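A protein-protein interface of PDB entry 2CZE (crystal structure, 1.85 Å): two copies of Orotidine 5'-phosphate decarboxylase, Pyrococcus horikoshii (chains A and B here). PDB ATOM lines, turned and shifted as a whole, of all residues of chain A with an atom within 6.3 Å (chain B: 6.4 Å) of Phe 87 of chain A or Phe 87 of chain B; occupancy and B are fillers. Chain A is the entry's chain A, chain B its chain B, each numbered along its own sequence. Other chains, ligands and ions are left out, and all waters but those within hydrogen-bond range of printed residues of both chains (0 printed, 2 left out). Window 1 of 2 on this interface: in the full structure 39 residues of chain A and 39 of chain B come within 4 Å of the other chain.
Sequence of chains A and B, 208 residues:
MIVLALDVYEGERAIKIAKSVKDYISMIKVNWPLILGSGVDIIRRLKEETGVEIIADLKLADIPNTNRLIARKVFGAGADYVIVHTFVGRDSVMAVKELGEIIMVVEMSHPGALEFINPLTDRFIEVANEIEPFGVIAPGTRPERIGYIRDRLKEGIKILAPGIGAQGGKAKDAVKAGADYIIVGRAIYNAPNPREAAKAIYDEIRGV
O of Ala 61 of chain B is in hydrogen-bond range of NE2 of His 85 of chain A (2.9 Å).
O of Gly 112 of chain A lies close to O of Val 88 of chain B (3.3 Å).
The backbone carbonyl oxygen (O) of Val 88 of chain A lies close to the backbone carbonyl oxygen (O) of Gly 112 of chain B (3.4 Å).
A ring nitrogen (NE2) of His 85 of chain B sits at hydrogen-bond distance from the backbone carbonyl oxygen (O) of Ala 61 of chain A, 2.8 Å away.
The backbone carbonyl oxygen (O) of Val 105 of chain B lies within hydrogen-bond range of the side-chain hydroxyl (OG1) of Thr 86 of chain B (2.7 Å).
The side-chain hydroxyl (OG1) of Thr 86 of chain A sits at hydrogen-bond distance from the backbone carbonyl oxygen (O) of Val 105 of chain A (2.8 Å).
Among the printed residues, merely in contact across the chains: Ala 61 of chain A with Met 108 of chain B (3.7 Å), Thr 86 of chain A with Phe 116 of chain B (3.9 Å), Phe 87 of chain A with His 85 of chain B (3.5 Å), Phe 87 of chain A with Phe 87 of chain B (3.5 Å), Phe 87 of chain A with Phe 116 of chain B (3.5 Å), Phe 87 of chain A with Ile 117 of chain B (3.8 Å), Val 88 of chain A with Ala 113 of chain B (3.9 Å), Gly 89 of chain A with Gly 112 of chain B (3.6 Å), Gly 89 of chain A with Glu 115 of chain B (3.4 Å), Gly 112 of chain A with Gly 89 of chain B (3.7 Å), Ala 113 of chain A with Val 88 of chain B (3.8 Å), Glu 115 of chain A with Gly 89 of chain B (3.3 Å), Phe 116 of chain A with Thr 86 of chain B (3.98 Å), Phe 116 of chain A with Phe 87 of chain B (3.5 Å), Phe 116 of chain A with Phe 124 of chain B (3.7 Å), Ile 117 of chain A with Phe 87 of chain B (3.9 Å), Leu 120 of chain A with Phe 87 of chain B (3.7 Å) and Phe 124 of chain A with Phe 116 of chain B (3.7 Å).
Phe 87 of chain A touches just these residues of chain B: His 85, Phe 87, Phe 116 and Ile 117.
Of the printed residues of chain A, Ala 61 of chain B touches His 85 (2.9 Å).
Phe 87 of chain B touches just these residues of chain A: Phe 87, Phe 116, Ile 117 and Leu 120.
Printed residues of chain A within 4 Å of Ala 113 of chain B: Val 88 (3.9 Å).
Of the printed residues of chain A, Phe 124 of chain B touches Phe 116.
The nearest residue of chain B that does not touch Phe 87 of chain A is Val 88 of chain B (4.1 Å).
The nearest residue of chain A that does not touch Phe 87 of chain B is Phe 124 of chain A (4.1 Å).
Printed residues of chain A that touch a printed residue of chain B: Ala 61, His 85, Thr 86, Phe 87, Val 88, Gly 89, Gly 112, Ala 113, Glu 115, Phe 116, Ile 117, Leu 120 and Phe 124.
Hydrophobic or aromatic side chains of chain A that line the printed part of chain B: Ala 61, His 85, Phe 87, Phe 116, Ile 117, Leu 120 and Phe 124.
Printed residues of chain B that touch a printed residue of chain A: Ala 61, His 85, Thr 86, Phe 87, Val 88, Gly 89, Met 108, Gly 112, Ala 113, Glu 115, Phe 116, Ile 117 and Phe 124.
Among the printed residues, 22 pairs touch across the chains.
Among the printed residues, no Asp or Glu carboxylate lies within 4 Å of a Lys or Arg side-chain nitrogen of the other chain.
Ala 61 of chain A touches His 85 of chain B, and with the chains exchanged His 85 of chain A touches Ala 61 of chain B.
Thr 86 of chain A touches Phe 116 of chain B, and with the chains exchanged Phe 116 of chain A touches Thr 86 of chain B.
Phe 87 of chain A touches His 85 of chain B, but with the chains exchanged His 85 of chain A does not touch Phe 87 of chain B (6.8 Å).
Phe 116 of chain A touches Phe 124 of chain B, and with the chains exchanged Phe 124 of chain A touches Phe 116 of chain B.
15 positions are printed for both chains.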
ATOM      1  N   ALA A  61      -5.124   2.854   2.056  1.00  0.00           N
ATOM      2  CA  ALA A  61      -5.660   3.900   2.900  1.00  0.00           C
ATOM      3  C   ALA A  61      -5.232   5.278   2.401  1.00  0.00           C
ATOM      4  O   ALA A  61      -4.756   6.117   3.179  1.00  0.00           O
ATOM      5  CB  ALA A  61      -5.154   3.668   4.328  1.00  0.00           C
ATOM      6  N   HIS A  85      -8.569  -0.422   3.907  1.00  0.00           N
ATOM      7  CA  HIS A  85      -9.044   0.077   5.183  1.00  0.00           C
ATOM      8  C   HIS A  85     -10.398   0.741   4.970  1.00  0.00           C
ATOM      9  O   HIS A  85     -10.696   1.212   3.868  1.00  0.00           O
ATOM     10  CB  HIS A  85      -8.077   1.106   5.745  1.00  0.00           C
ATOM     11  CG  HIS A  85      -7.093   0.537   6.711  1.00  0.00           C
ATOM     12  ND1 HIS A  85      -7.470  -0.005   7.920  1.00  0.00           N
ATOM     13  CD2 HIS A  85      -5.746   0.432   6.653  1.00  0.00           C
ATOM     14  CE1 HIS A  85      -6.394  -0.420   8.566  1.00  0.00           C
ATOM     15  NE2 HIS A  85      -5.335  -0.166   7.818  1.00  0.00           N
ATOM     16  N   THR A  86     -11.211   0.768   6.021  1.00  0.00           N
ATOM     17  CA  THR A  86     -12.515   1.403   5.955  1.00  0.00           C
ATOM     18  C   THR A  86     -12.441   2.829   6.522  1.00  0.00           C
ATOM     19  O   THR A  86     -13.194   3.715   6.095  1.00  0.00           O
ATOM     20  CB  THR A  86     -13.580   0.620   6.785  1.00  0.00           C
ATOM     21  OG1 THR A  86     -13.629  -0.752   6.353  1.00  0.00           O
ATOM     22  CG2 THR A  86     -14.964   1.250   6.591  1.00  0.00           C
ATOM     23  N   PHE A  87     -11.517   3.058   7.458  1.00  0.00           N
ATOM     24  CA  PHE A  87     -11.441   4.371   8.106  1.00  0.00           C
ATOM     25  C   PHE A  87     -11.152   5.582   7.218  1.00  0.00           C
ATOM     26  O   PHE A  87     -11.462   6.705   7.598  1.00  0.00           O
ATOM     27  CB  PHE A  87     -10.471   4.345   9.313  1.00  0.00           C
ATOM     28  CG  PHE A  87      -8.999   4.378   8.954  1.00  0.00           C
ATOM     29  CD1 PHE A  87      -8.229   3.210   8.982  1.00  0.00           C
ATOM     30  CD2 PHE A  87      -8.363   5.589   8.670  1.00  0.00           C
ATOM     31  CE1 PHE A  87      -6.840   3.252   8.739  1.00  0.00           C
ATOM     32  CE2 PHE A  87      -6.970   5.641   8.424  1.00  0.00           C
ATOM     33  CZ  PHE A  87      -6.216   4.478   8.462  1.00  0.00           C
ATOM     34  N   VAL A  88     -10.580   5.359   6.039  1.00  0.00           N
ATOM     35  CA  VAL A  88     -10.264   6.459   5.135  1.00  0.00           C
ATOM     36  C   VAL A  88     -11.508   6.937   4.367  1.00  0.00           C
ATOM     37  O   VAL A  88     -11.464   7.926   3.640  1.00  0.00           O
ATOM     38  CB  VAL A  88      -9.106   6.045   4.181  1.00  0.00           C
ATOM     39  CG1 VAL A  88      -8.896   7.070   3.100  1.00  0.00           C
ATOM     40  CG2 VAL A  88      -7.826   5.923   4.990  1.00  0.00           C
ATOM     41  N   GLY A  89     -12.629   6.243   4.553  1.00  0.00           N
ATOM     42  CA  GLY A  89     -13.858   6.664   3.903  1.00  0.00           C
ATOM     43  C   GLY A  89     -14.354   5.847   2.738  1.00  0.00           C
ATOM     44  O   GLY A  89     -13.589   5.145   2.075  1.00  0.00           O
ATOM     45  N   VAL A  93     -12.637   3.398  -0.684  1.00  0.00           N
ATOM     46  CA  VAL A  93     -12.970   1.979  -0.753  1.00  0.00           C
ATOM     47  C   VAL A  93     -13.521   1.647  -2.140  1.00  0.00           C
ATOM     48  O   VAL A  93     -13.106   0.669  -2.773  1.00  0.00           O
ATOM     49  CB  VAL A  93     -14.053   1.589   0.300  1.00  0.00           C
ATOM     50  CG1 VAL A  93     -14.445   0.111   0.122  1.00  0.00           C
ATOM     51  CG2 VAL A  93     -13.514   1.819   1.733  1.00  0.00           C
ATOM     52  N   VAL A 105     -11.234  -3.799   6.163  1.00  0.00           N
ATOM     53  CA  VAL A 105     -10.804  -3.938   7.548  1.00  0.00           C
ATOM     54  C   VAL A 105     -11.922  -3.412   8.458  1.00  0.00           C
ATOM     55  O   VAL A 105     -12.380  -2.279   8.297  1.00  0.00           O
ATOM     56  CB  VAL A 105      -9.539  -3.110   7.826  1.00  0.00           C
ATOM     57  CG1 VAL A 105      -9.131  -3.271   9.304  1.00  0.00           C
ATOM     58  CG2 VAL A 105      -8.398  -3.559   6.905  1.00  0.00           C
ATOM     59  N   GLY A 112      -2.911  -1.733  19.522  1.00  0.00           N
ATOM     60  CA  GLY A 112      -3.239  -0.391  19.072  1.00  0.00           C
ATOM     61  C   GLY A 112      -4.610  -0.270  18.436  1.00  0.00           C
ATOM     62  O   GLY A 112      -5.168   0.829  18.354  1.00  0.00           O
ATOM     63  N   ALA A 113      -5.163  -1.392  17.989  1.00  0.00           N
ATOM     64  CA  ALA A 113      -6.477  -1.380  17.350  1.00  0.00           C
ATOM     65  C   ALA A 113      -7.578  -0.919  18.309  1.00  0.00           C
ATOM     66  O   ALA A 113      -8.662  -0.501  17.877  1.00  0.00           O
ATOM     67  CB  ALA A 113      -6.811  -2.771  16.829  1.00  0.00           C
ATOM     68  N   GLU A 115      -7.364   1.620  20.315  1.00  0.00           N
ATOM     69  CA  GLU A 115      -7.341   3.065  20.469  1.00  0.00           C
ATOM     70  C   GLU A 115      -8.380   3.830  19.646  1.00  0.00           C
ATOM     71  O   GLU A 115      -9.110   4.669  20.187  1.00  0.00           O
ATOM     72  CB  GLU A 115      -5.926   3.591  20.181  1.00  0.00           C
ATOM     73  CG  GLU A 115      -4.998   3.424  21.373  1.00  0.00           C
ATOM     74  CD  GLU A 115      -3.521   3.466  21.018  1.00  0.00           C
ATOM     75  OE1 GLU A 115      -3.146   4.156  20.048  1.00  0.00           O
ATOM     76  OE2 GLU A 115      -2.729   2.812  21.736  1.00  0.00           O
ATOM     77  N   PHE A 116      -8.470   3.537  18.355  1.00  0.00           N
ATOM     78  CA  PHE A 116      -9.423   4.244  17.499  1.00  0.00           C
ATOM     79  C   PHE A 116     -10.347   3.370  16.658  1.00  0.00           C
ATOM     80  O   PHE A 116     -11.472   3.759  16.353  1.00  0.00           O
ATOM     81  CB  PHE A 116      -8.672   5.194  16.556  1.00  0.00           C
ATOM     82  CG  PHE A 116      -7.870   6.238  17.262  1.00  0.00           C
ATOM     83  CD1 PHE A 116      -6.479   6.143  17.328  1.00  0.00           C
ATOM     84  CD2 PHE A 116      -8.504   7.321  17.868  1.00  0.00           C
ATOM     85  CE1 PHE A 116      -5.727   7.121  17.994  1.00  0.00           C
ATOM     86  CE2 PHE A 116      -7.765   8.303  18.534  1.00  0.00           C
ATOM     87  CZ  PHE A 116      -6.374   8.206  18.598  1.00  0.00           C
ATOM     88  N   ILE A 117      -9.865   2.202  16.257  1.00  0.00           N
ATOM     89  CA  ILE A 117     -10.653   1.315  15.416  1.00  0.00           C
ATOM     90  C   ILE A 117     -11.784   0.584  16.139  1.00  0.00           C
ATOM     91  O   ILE A 117     -12.949   0.660  15.732  1.00  0.00           O
ATOM     92  CB  ILE A 117      -9.732   0.287  14.727  1.00  0.00           C
ATOM     93  CG1 ILE A 117      -8.846   1.008  13.696  1.00  0.00           C
ATOM     94  CG2 ILE A 117     -10.566  -0.807  14.076  1.00  0.00           C
ATOM     95  CD1 ILE A 117      -7.786   0.124  13.058  1.00  0.00           C
ATOM     96  N   LEU A 120     -15.088   2.131  16.856  1.00  0.00           N
ATOM     97  CA  LEU A 120     -15.928   2.426  15.691  1.00  0.00           C
ATOM     98  C   LEU A 120     -16.394   1.180  14.946  1.00  0.00           C
ATOM     99  O   LEU A 120     -16.964   1.279  13.856  1.00  0.00           O
ATOM    100  CB  LEU A 120     -15.164   3.330  14.716  1.00  0.00           C
ATOM    101  CG  LEU A 120     -15.009   4.789  15.145  1.00  0.00           C
ATOM    102  CD1 LEU A 120     -13.962   5.501  14.297  1.00  0.00           C
ATOM    103  CD2 LEU A 120     -16.363   5.459  14.996  1.00  0.00           C
ATOM    104  N   PHE A 124     -18.167   0.659  11.156  1.00  0.00           N
ATOM    105  CA  PHE A 124     -17.469  -0.008  10.055  1.00  0.00           C
ATOM    106  C   PHE A 124     -18.294  -1.173   9.492  1.00  0.00           C
ATOM    107  O   PHE A 124     -18.317  -1.406   8.282  1.00  0.00           O
ATOM    108  CB  PHE A 124     -16.088  -0.497  10.530  1.00  0.00           C
ATOM    109  CG  PHE A 124     -15.130   0.624  10.870  1.00  0.00           C
ATOM    110  CD1 PHE A 124     -14.141   0.449  11.834  1.00  0.00           C
ATOM    111  CD2 PHE A 124     -15.228   1.856  10.226  1.00  0.00           C
ATOM    112  CE1 PHE A 124     -13.258   1.492  12.156  1.00  0.00           C
ATOM    113  CE2 PHE A 124     -14.353   2.905  10.536  1.00  0.00           C
ATOM    114  CZ  PHE A 124     -13.361   2.721  11.510  1.00  0.00           C
ATOM    115  N   ALA B  61      -0.236   1.258   7.789  1.00  0.00           N
ATOM    116  CA  ALA B  61      -1.422   1.074   8.606  1.00  0.00           C
ATOM    117  C   ALA B  61      -1.619  -0.388   8.960  1.00  0.00           C
ATOM    118  O   ALA B  61      -2.740  -0.902   8.878  1.00  0.00           O
ATOM    119  CB  ALA B  61      -2.633   1.589   7.811  1.00  0.00           C
ATOM    120  N   HIS B  85      -0.046   6.202   9.156  1.00  0.00           N
ATOM    121  CA  HIS B  85      -1.344   6.622   9.658  1.00  0.00           C
ATOM    122  C   HIS B  85      -1.312   6.622  11.179  1.00  0.00           C
ATOM    123  O   HIS B  85      -0.536   5.891  11.782  1.00  0.00           O
ATOM    124  CB  HIS B  85      -2.453   5.673   9.173  1.00  0.00           C
ATOM    125  CG  HIS B  85      -3.100   6.109   7.894  1.00  0.00           C
ATOM    126  ND1 HIS B  85      -3.875   7.245   7.805  1.00  0.00           N
ATOM    127  CD2 HIS B  85      -3.102   5.555   6.657  1.00  0.00           C
ATOM    128  CE1 HIS B  85      -4.330   7.373   6.570  1.00  0.00           C
ATOM    129  NE2 HIS B  85      -3.876   6.360   5.852  1.00  0.00           N
ATOM    130  N   THR B  86      -2.173   7.431  11.787  1.00  0.00           N
ATOM    131  CA  THR B  86      -2.256   7.504  13.240  1.00  0.00           C
ATOM    132  C   THR B  86      -3.424   6.625  13.708  1.00  0.00           C
ATOM    133  O   THR B  86      -3.400   6.070  14.809  1.00  0.00           O
ATOM    134  CB  THR B  86      -2.506   8.971  13.707  1.00  0.00           C
ATOM    135  OG1 THR B  86      -1.522   9.832  13.123  1.00  0.00           O
ATOM    136  CG2 THR B  86      -2.405   9.085  15.242  1.00  0.00           C
ATOM    137  N   PHE B  87      -4.432   6.478  12.850  1.00  0.00           N
ATOM    138  CA  PHE B  87      -5.645   5.718  13.172  1.00  0.00           C
ATOM    139  C   PHE B  87      -5.408   4.299  13.705  1.00  0.00           C
ATOM    140  O   PHE B  87      -6.176   3.796  14.515  1.00  0.00           O
ATOM    141  CB  PHE B  87      -6.522   5.603  11.925  1.00  0.00           C
ATOM    142  CG  PHE B  87      -7.990   5.784  12.182  1.00  0.00           C
ATOM    143  CD1 PHE B  87      -8.618   6.996  11.885  1.00  0.00           C
ATOM    144  CD2 PHE B  87      -8.761   4.737  12.682  1.00  0.00           C
ATOM    145  CE1 PHE B  87      -9.995   7.160  12.080  1.00  0.00           C
ATOM    146  CE2 PHE B  87     -10.143   4.896  12.883  1.00  0.00           C
ATOM    147  CZ  PHE B  87     -10.752   6.113  12.578  1.00  0.00           C
ATOM    148  N   VAL B  88      -4.355   3.650  13.224  1.00  0.00           N
ATOM    149  CA  VAL B  88      -4.073   2.277  13.606  1.00  0.00           C
ATOM    150  C   VAL B  88      -3.500   2.103  15.009  1.00  0.00           C
ATOM    151  O   VAL B  88      -3.423   0.984  15.517  1.00  0.00           O
ATOM    152  CB  VAL B  88      -3.176   1.616  12.508  1.00  0.00           C
ATOM    153  CG1 VAL B  88      -2.765   0.216  12.902  1.00  0.00           C
ATOM    154  CG2 VAL B  88      -3.980   1.563  11.198  1.00  0.00           C
ATOM    155  N   GLY B  89      -3.123   3.203  15.650  1.00  0.00           N
ATOM    156  CA  GLY B  89      -2.623   3.088  17.013  1.00  0.00           C
ATOM    157  C   GLY B  89      -1.194   3.496  17.226  1.00  0.00           C
ATOM    158  O   GLY B  89      -0.381   3.466  16.302  1.00  0.00           O
ATOM    159  N   VAL B  93       2.649   3.147  15.094  1.00  0.00           N
ATOM    160  CA  VAL B  93       3.415   4.327  14.708  1.00  0.00           C
ATOM    161  C   VAL B  93       4.850   4.213  15.231  1.00  0.00           C
ATOM    162  O   VAL B  93       5.817   4.452  14.490  1.00  0.00           O
ATOM    163  CB  VAL B  93       2.799   5.633  15.280  1.00  0.00           C
ATOM    164  CG1 VAL B  93       3.673   6.823  14.928  1.00  0.00           C
ATOM    165  CG2 VAL B  93       1.391   5.828  14.715  1.00  0.00           C
ATOM    166  N   VAL B 105      -0.228  11.077   9.700  1.00  0.00           N
ATOM    167  CA  VAL B 105      -1.422  11.618   9.069  1.00  0.00           C
ATOM    168  C   VAL B 105      -2.328  12.116  10.193  1.00  0.00           C
ATOM    169  O   VAL B 105      -2.587  11.374  11.135  1.00  0.00           O
ATOM    170  CB  VAL B 105      -2.187  10.536   8.251  1.00  0.00           C
ATOM    171  CG1 VAL B 105      -3.469  11.140   7.648  1.00  0.00           C
ATOM    172  CG2 VAL B 105      -1.299   9.998   7.132  1.00  0.00           C
ATOM    173  N   MET B 108      -6.834  14.043   6.340  1.00  0.00           N
ATOM    174  CA  MET B 108      -6.610  13.877   4.902  1.00  0.00           C
ATOM    175  C   MET B 108      -7.405  14.885   4.072  1.00  0.00           C
ATOM    176  O   MET B 108      -8.343  15.502   4.567  1.00  0.00           O
ATOM    177  CB  MET B 108      -6.925  12.435   4.485  1.00  0.00           C
ATOM    178  CG  MET B 108      -5.957  11.445   5.125  1.00  0.00           C
ATOM    179  SD  MET B 108      -6.184   9.719   4.631  1.00  0.00           S
ATOM    180  CE  MET B 108      -5.631   9.745   2.908  1.00  0.00           C
ATOM    181  N   GLY B 112     -13.747  11.632   1.564  1.00  0.00           N
ATOM    182  CA  GLY B 112     -13.890  10.536   2.504  1.00  0.00           C
ATOM    183  C   GLY B 112     -13.282  10.794   3.872  1.00  0.00           C
ATOM    184  O   GLY B 112     -13.670  10.171   4.857  1.00  0.00           O
ATOM    185  N   ALA B 113     -12.339  11.725   3.942  1.00  0.00           N
ATOM    186  CA  ALA B 113     -11.661  12.031   5.198  1.00  0.00           C
ATOM    187  C   ALA B 113     -12.619  12.594   6.225  1.00  0.00           C
ATOM    188  O   ALA B 113     -12.352  12.542   7.417  1.00  0.00           O
ATOM    189  CB  ALA B 113     -10.522  13.020   4.960  1.00  0.00           C
ATOM    190  N   GLU B 115     -15.573  11.423   6.921  1.00  0.00           N
ATOM    191  CA  GLU B 115     -16.367  10.371   7.560  1.00  0.00           C
ATOM    192  C   GLU B 115     -15.883   9.898   8.937  1.00  0.00           C
ATOM    193  O   GLU B 115     -16.657   9.877   9.896  1.00  0.00           O
ATOM    194  CB  GLU B 115     -16.497   9.176   6.608  1.00  0.00           C
ATOM    195  CG  GLU B 115     -17.461   9.444   5.443  1.00  0.00           C
ATOM    196  CD  GLU B 115     -17.376   8.402   4.327  1.00  0.00           C
ATOM    197  OE1 GLU B 115     -17.163   7.210   4.626  1.00  0.00           O
ATOM    198  OE2 GLU B 115     -17.543   8.782   3.148  1.00  0.00           O
ATOM    199  N   PHE B 116     -14.605   9.535   9.045  1.00  0.00           N
ATOM    200  CA  PHE B 116     -14.068   9.046  10.314  1.00  0.00           C
ATOM    201  C   PHE B 116     -12.846   9.780  10.844  1.00  0.00           C
ATOM    202  O   PHE B 116     -12.685   9.922  12.055  1.00  0.00           O
ATOM    203  CB  PHE B 116     -13.709   7.561  10.203  1.00  0.00           C
ATOM    204  CG  PHE B 116     -14.865   6.684   9.831  1.00  0.00           C
ATOM    205  CD1 PHE B 116     -14.977   6.160   8.544  1.00  0.00           C
ATOM    206  CD2 PHE B 116     -15.849   6.381  10.770  1.00  0.00           C
ATOM    207  CE1 PHE B 116     -16.051   5.346   8.203  1.00  0.00           C
ATOM    208  CE2 PHE B 116     -16.925   5.568  10.435  1.00  0.00           C
ATOM    209  CZ  PHE B 116     -17.027   5.050   9.153  1.00  0.00           C
ATOM    210  N   ILE B 117     -11.989  10.240   9.940  1.00  0.00           N
ATOM    211  CA  ILE B 117     -10.763  10.931  10.325  1.00  0.00           C
ATOM    212  C   ILE B 117     -10.981  12.335  10.889  1.00  0.00           C
ATOM    213  O   ILE B 117     -10.547  12.633  12.000  1.00  0.00           O
ATOM    214  CB  ILE B 117      -9.808  11.027   9.114  1.00  0.00           C
ATOM    215  CG1 ILE B 117      -9.337   9.628   8.715  1.00  0.00           C
ATOM    216  CG2 ILE B 117      -8.643  11.972   9.424  1.00  0.00           C
ATOM    217  CD1 ILE B 117      -8.519   9.620   7.425  1.00  0.00           C
ATOM    218  N   LEU B 120     -12.007  12.990  14.467  1.00  0.00           N
ATOM    219  CA  LEU B 120     -11.021  12.629  15.491  1.00  0.00           C
ATOM    220  C   LEU B 120      -9.748  13.465  15.438  1.00  0.00           C
ATOM    221  O   LEU B 120      -8.779  13.163  16.132  1.00  0.00           O
ATOM    222  CB  LEU B 120     -10.648  11.145  15.363  1.00  0.00           C
ATOM    223  CG  LEU B 120     -11.721  10.125  15.752  1.00  0.00           C
ATOM    224  CD1 LEU B 120     -11.350   8.746  15.215  1.00  0.00           C
ATOM    225  CD2 LEU B 120     -11.858  10.091  17.270  1.00  0.00           C
ATOM    226  N   PHE B 124      -5.972  13.073  17.214  1.00  0.00           N
ATOM    227  CA  PHE B 124      -4.772  12.787  16.422  1.00  0.00           C
ATOM    228  C   PHE B 124      -3.682  13.835  16.641  1.00  0.00           C
ATOM    229  O   PHE B 124      -2.492  13.518  16.638  1.00  0.00           O
ATOM    230  CB  PHE B 124      -5.135  12.685  14.943  1.00  0.00           C
ATOM    231  CG  PHE B 124      -6.036  11.528  14.627  1.00  0.00           C
ATOM    232  CD1 PHE B 124      -6.917  11.590  13.545  1.00  0.00           C
ATOM    233  CD2 PHE B 124      -6.003  10.370  15.403  1.00  0.00           C
ATOM    234  CE1 PHE B 124      -7.760  10.506  13.246  1.00  0.00           C
ATOM    235  CE2 PHE B 124      -6.836   9.291  15.112  1.00  0.00           C
ATOM    236  CZ  PHE B 124      -7.715   9.366  14.031  1.00  0.00           C
